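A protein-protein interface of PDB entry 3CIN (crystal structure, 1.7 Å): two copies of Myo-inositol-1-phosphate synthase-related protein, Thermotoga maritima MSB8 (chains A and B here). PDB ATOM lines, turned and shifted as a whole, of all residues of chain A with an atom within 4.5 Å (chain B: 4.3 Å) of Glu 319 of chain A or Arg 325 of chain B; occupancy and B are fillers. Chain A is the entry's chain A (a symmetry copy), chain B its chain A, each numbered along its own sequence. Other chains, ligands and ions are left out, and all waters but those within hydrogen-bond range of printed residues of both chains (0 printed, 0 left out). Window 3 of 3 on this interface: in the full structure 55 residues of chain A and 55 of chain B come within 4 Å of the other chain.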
ATOM      1  N   HIS A 307      20.390   2.839  19.258  1.00  0.00           N
ATOM      2  CA  HIS A 307      20.597   3.106  20.657  1.00  0.00           C
ATOM      3  C   HIS A 307      21.447   4.326  20.789  1.00  0.00           C
ATOM      4  O   HIS A 307      22.526   4.418  20.196  1.00  0.00           O
ATOM      5  CB  HIS A 307      21.355   1.970  21.293  1.00  0.00           C
ATOM      6  CG  HIS A 307      21.709   2.194  22.738  1.00  0.00           C
ATOM      7  ND1 HIS A 307      22.983   2.517  23.156  1.00  0.00           N
ATOM      8  CD2 HIS A 307      20.947   2.151  23.851  1.00  0.00           C
ATOM      9  CE1 HIS A 307      22.980   2.664  24.469  1.00  0.00           C
ATOM     10  NE2 HIS A 307      21.760   2.441  24.915  1.00  0.00           N
ATOM     11  N   ILE A 308      20.977   5.274  21.601  1.00  0.00           N
ATOM     12  CA  ILE A 308      21.721   6.541  21.804  1.00  0.00           C
ATOM     13  C   ILE A 308      21.709   6.794  23.275  1.00  0.00           C
ATOM     14  O   ILE A 308      20.686   6.677  23.918  1.00  0.00           O
ATOM     15  CB  ILE A 308      21.089   7.721  21.004  1.00  0.00           C
ATOM     16  CG1 ILE A 308      21.239   7.463  19.507  1.00  0.00           C
ATOM     17  CG2 ILE A 308      21.786   9.051  21.310  1.00  0.00           C
ATOM     18  CD1 ILE A 308      20.388   8.408  18.602  1.00  0.00           C
ATOM     19  N   GLU A 309      22.884   7.072  23.841  1.00  0.00           N
ATOM     20  CA  GLU A 309      22.955   7.507  25.213  1.00  0.00           C
ATOM     21  C   GLU A 309      23.579   8.870  25.310  1.00  0.00           C
ATOM     22  O   GLU A 309      24.450   9.227  24.526  1.00  0.00           O
ATOM     23  CB  GLU A 309      23.621   6.515  26.143  1.00  0.00           C
ATOM     24  CG  GLU A 309      24.860   6.021  25.784  1.00  0.00           C
ATOM     25  CD  GLU A 309      25.404   5.065  26.858  1.00  0.00           C
ATOM     26  OE1 GLU A 309      24.632   4.651  27.777  1.00  0.00           O
ATOM     27  OE2 GLU A 309      26.615   4.757  26.776  1.00  0.00           O
ATOM     28  N   TYR A 310      23.062   9.656  26.236  1.00  0.00           N
ATOM     29  CA  TYR A 310      23.439  11.051  26.308  1.00  0.00           C
ATOM     30  C   TYR A 310      23.413  11.571  27.715  1.00  0.00           C
ATOM     31  O   TYR A 310      22.774  11.009  28.592  1.00  0.00           O
ATOM     32  CB  TYR A 310      22.547  11.888  25.395  1.00  0.00           C
ATOM     33  CG  TYR A 310      21.062  11.803  25.697  1.00  0.00           C
ATOM     34  CD1 TYR A 310      20.242  10.844  25.082  1.00  0.00           C
ATOM     35  CD2 TYR A 310      20.470  12.733  26.559  1.00  0.00           C
ATOM     36  CE1 TYR A 310      18.927  10.794  25.415  1.00  0.00           C
ATOM     37  CE2 TYR A 310      19.122  12.698  26.839  1.00  0.00           C
ATOM     38  CZ  TYR A 310      18.363  11.734  26.238  1.00  0.00           C
ATOM     39  OH  TYR A 310      17.017  11.684  26.551  1.00  0.00           O
ATOM     40  N   ASP A 318      20.833   9.484  30.164  1.00  0.00           N
ATOM     41  CA  ASP A 318      19.566   8.989  29.595  1.00  0.00           C
ATOM     42  C   ASP A 318      19.898   8.086  28.415  1.00  0.00           C
ATOM     43  O   ASP A 318      20.981   8.160  27.851  1.00  0.00           O
ATOM     44  CB  ASP A 318      18.693  10.121  29.114  1.00  0.00           C
ATOM     45  CG  ASP A 318      18.156  11.030  30.251  1.00  0.00           C
ATOM     46  OD1 ASP A 318      18.232  10.692  31.434  1.00  0.00           O
ATOM     47  OD2 ASP A 318      17.572  12.088  29.921  1.00  0.00           O
ATOM     48  N   GLU A 319      18.942   7.250  28.014  1.00  0.00           N
ATOM     49  CA  GLU A 319      19.135   6.334  26.925  1.00  0.00           C
ATOM     50  C   GLU A 319      17.845   6.249  26.119  1.00  0.00           C
ATOM     51  O   GLU A 319      16.774   6.119  26.745  1.00  0.00           O
ATOM     52  CB  GLU A 319      19.287   4.962  27.584  1.00  0.00           C
ATOM     53  CG  GLU A 319      20.227   4.093  27.019  1.00  0.00           C
ATOM     54  CD  GLU A 319      20.556   2.991  27.980  1.00  0.00           C
ATOM     55  OE1 GLU A 319      20.029   2.986  29.120  1.00  0.00           O
ATOM     56  OE2 GLU A 319      21.366   2.143  27.590  1.00  0.00           O
ATOM     57  N   LEU A 320      17.960   6.196  24.781  1.00  0.00           N
ATOM     58  CA  LEU A 320      16.837   5.968  23.875  1.00  0.00           C
ATOM     59  C   LEU A 320      17.119   4.732  23.051  1.00  0.00           C
ATOM     60  O   LEU A 320      18.222   4.641  22.550  1.00  0.00           O
ATOM     61  CB  LEU A 320      16.640   7.138  22.948  1.00  0.00           C
ATOM     62  CG  LEU A 320      16.233   8.410  23.643  1.00  0.00           C
ATOM     63  CD1 LEU A 320      16.429   9.606  22.694  1.00  0.00           C
ATOM     64  CD2 LEU A 320      14.732   8.280  24.188  1.00  0.00           C
ATOM     65  N   MET A 321      16.153   3.781  22.955  1.00  0.00           N
ATOM     66  CA  MET A 321      16.275   2.596  22.048  1.00  0.00           C
ATOM     67  C   MET A 321      15.106   2.682  21.034  1.00  0.00           C
ATOM     68  O   MET A 321      13.961   2.597  21.474  1.00  0.00           O
ATOM     69  CB  MET A 321      16.278   1.249  22.780  1.00  0.00           C
ATOM     70  CG  MET A 321      17.176   1.173  24.084  1.00  0.00           C
ATOM     71  SD  MET A 321      17.350  -0.294  25.138  1.00  0.00           S
ATOM     72  CE  MET A 321      18.588   0.282  26.312  1.00  0.00           C
ATOM     73  N   LEU B 298      11.618   2.734  40.060  1.00  0.00           N
ATOM     74  CA  LEU B 298      12.150   3.470  38.926  1.00  0.00           C
ATOM     75  C   LEU B 298      12.678   4.802  39.406  1.00  0.00           C
ATOM     76  O   LEU B 298      13.477   5.414  38.700  1.00  0.00           O
ATOM     77  CB  LEU B 298      11.099   3.703  37.843  1.00  0.00           C
ATOM     78  CG  LEU B 298      10.673   2.393  37.142  1.00  0.00           C
ATOM     79  CD1 LEU B 298       9.518   2.730  36.239  1.00  0.00           C
ATOM     80  CD2 LEU B 298      11.788   1.777  36.276  1.00  0.00           C
ATOM     81  N   LYS B 301      13.823   8.156  37.304  1.00  0.00           N
ATOM     82  CA  LYS B 301      14.156   7.801  35.914  1.00  0.00           C
ATOM     83  C   LYS B 301      13.018   7.025  35.230  1.00  0.00           C
ATOM     84  O   LYS B 301      12.946   5.817  35.395  1.00  0.00           O
ATOM     85  CB  LYS B 301      15.463   7.028  35.857  1.00  0.00           C
ATOM     86  CG  LYS B 301      16.185   7.014  34.463  1.00  0.00           C
ATOM     87  CD  LYS B 301      17.592   6.317  34.528  1.00  0.00           C
ATOM     88  CE  LYS B 301      18.308   6.444  33.146  1.00  0.00           C
ATOM     89  NZ  LYS B 301      19.575   5.652  33.028  1.00  0.00           N
ATOM     90  N   LYS B 302      12.235   7.753  34.448  1.00  0.00           N
ATOM     91  CA  LYS B 302      11.026   7.237  33.783  1.00  0.00           C
ATOM     92  C   LYS B 302      11.377   6.178  32.796  1.00  0.00           C
ATOM     93  O   LYS B 302      12.457   6.223  32.214  1.00  0.00           O
ATOM     94  CB  LYS B 302      10.310   8.353  33.013  1.00  0.00           C
ATOM     95  CG  LYS B 302       9.557   9.306  33.810  1.00  0.00           C
ATOM     96  CD  LYS B 302       8.636  10.040  32.851  1.00  0.00           C
ATOM     97  CE  LYS B 302       7.742  11.013  33.535  1.00  0.00           C
ATOM     98  NZ  LYS B 302       7.364  12.065  32.568  1.00  0.00           N
ATOM     99  N   PHE B 303      10.496   5.182  32.635  1.00  0.00           N
ATOM    100  CA  PHE B 303      10.538   4.303  31.484  1.00  0.00           C
ATOM    101  C   PHE B 303       9.463   4.814  30.548  1.00  0.00           C
ATOM    102  O   PHE B 303       8.351   5.082  30.977  1.00  0.00           O
ATOM    103  CB  PHE B 303      10.257   2.857  31.833  1.00  0.00           C
ATOM    104  CG  PHE B 303      10.074   1.981  30.639  1.00  0.00           C
ATOM    105  CD1 PHE B 303      11.134   1.702  29.769  1.00  0.00           C
ATOM    106  CD2 PHE B 303       8.816   1.414  30.359  1.00  0.00           C
ATOM    107  CE1 PHE B 303      10.948   0.882  28.655  1.00  0.00           C
ATOM    108  CE2 PHE B 303       8.635   0.567  29.259  1.00  0.00           C
ATOM    109  CZ  PHE B 303       9.703   0.329  28.376  1.00  0.00           C
ATOM    110  N   GLY B 324      12.690   4.227  26.190  1.00  0.00           N
ATOM    111  CA  GLY B 324      13.725   5.118  26.753  1.00  0.00           C
ATOM    112  C   GLY B 324      13.739   5.030  28.240  1.00  0.00           C
ATOM    113  O   GLY B 324      12.754   4.609  28.854  1.00  0.00           O
ATOM    114  N   ARG B 325      14.862   5.431  28.820  1.00  0.00           N
ATOM    115  CA  ARG B 325      14.937   5.676  30.260  1.00  0.00           C
ATOM    116  C   ARG B 325      15.443   7.079  30.346  1.00  0.00           C
ATOM    117  O   ARG B 325      16.586   7.340  29.948  1.00  0.00           O
ATOM    118  CB  ARG B 325      15.937   4.754  30.897  1.00  0.00           C
ATOM    119  CG  ARG B 325      15.501   3.331  30.936  1.00  0.00           C
ATOM    120  CD  ARG B 325      14.259   3.120  31.879  1.00  0.00           C
ATOM    121  NE  ARG B 325      14.263   3.666  33.252  1.00  0.00           N
ATOM    122  CZ  ARG B 325      14.811   3.094  34.337  1.00  0.00           C
ATOM    123  NH1 ARG B 325      15.505   1.994  34.220  1.00  0.00           N
ATOM    124  NH2 ARG B 325      14.694   3.621  35.546  1.00  0.00           N
ATOM    125  N   ILE B 326      14.641   7.932  30.918  1.00  0.00           N
ATOM    126  CA  ILE B 326      14.928   9.365  30.989  1.00  0.00           C
ATOM    127  C   ILE B 326      14.781   9.926  32.418  1.00  0.00           C
ATOM    128  O   ILE B 326      13.783   9.709  33.109  1.00  0.00           O
ATOM    129  CB  ILE B 326      14.143  10.141  29.957  1.00  0.00           C
ATOM    130  CG1 ILE B 326      12.653   9.933  30.074  1.00  0.00           C
ATOM    131  CG2 ILE B 326      14.461   9.657  28.503  1.00  0.00           C
ATOM    132  CD1 ILE B 326      11.957  10.481  28.848  1.00  0.00           C
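Printed residues of chain B within 4 Å of Tyr 310 of chain A: Ile 326. Printed residues of chain B within 4 Å of Asp 318 of chain A: Arg 325 and Ile 326. Glu 319 of chain A touches just these residues of chain B: Gly 324 and Arg 325. Arg 325 of chain B touches two residues of chain A. Of the printed residues of chain A, Ile 326 of chain B touches Tyr 310 (3.8 Å) and Asp 318 (3.6 Å). The nearest printed residue of chain A that does not touch Arg 325 of chain B is Leu 320 of chain A (5.1 Å). The nearest printed residue of chain B that does not touch Asp 318 of chain A is Lys 301 of chain B (4.5 Å).
No position is printed for both chains.
The backbone carbonyl oxygen (O) of Lys 301 of chain B is in hydrogen-bond range of the guanidinium group (NH2) of Arg 325 of chain B (2.8 Å). The backbone carbonyl oxygen of Lys 302 of chain B sits close to the guanidinium group of Arg 325 of chain B (3.3 Å). O of Ile 326 of chain B is in hydrogen-bond range of N of Lys 302 of chain B (2.8 Å). OE2 of Glu 319 of chain A sits at hydrogen-bond distance from NE2 of His 307 of chain A (2.7 Å). The backbone carbonyl oxygen (O) of Tyr 310 of chain A sits at hydrogen-bond distance from the backbone NH (N) of Asp 318 of chain A (2.9 Å).
The backbone NH (N) of Arg 325 of chain B sits at hydrogen-bond distance from the backbone carbonyl oxygen (O) of Glu 319 of chain A, 2.9 Å away.
Printed residues of chain A that touch a printed residue of chain B: Tyr 310, Asp 318 and Glu 319. Hydrophobic or aromatic side chains of chain A that line the printed part of chain B: Tyr 310. Among the printed residues, no Asp or Glu carboxylate lies within 4 Å of a Lys or Arg side-chain nitrogen of the other chain.
Among the printed residues, merely in contact across the chains: Tyr 310 of chain A with Ile 326 of chain B (3.8 Å), Asp 318 of chain A with Arg 325 of chain B (3.4 Å), Asp 318 of chain A with Ile 326 of chain B (3.6 Å) and Glu 319 of chain A with Gly 324 of chain B (3.2 Å).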
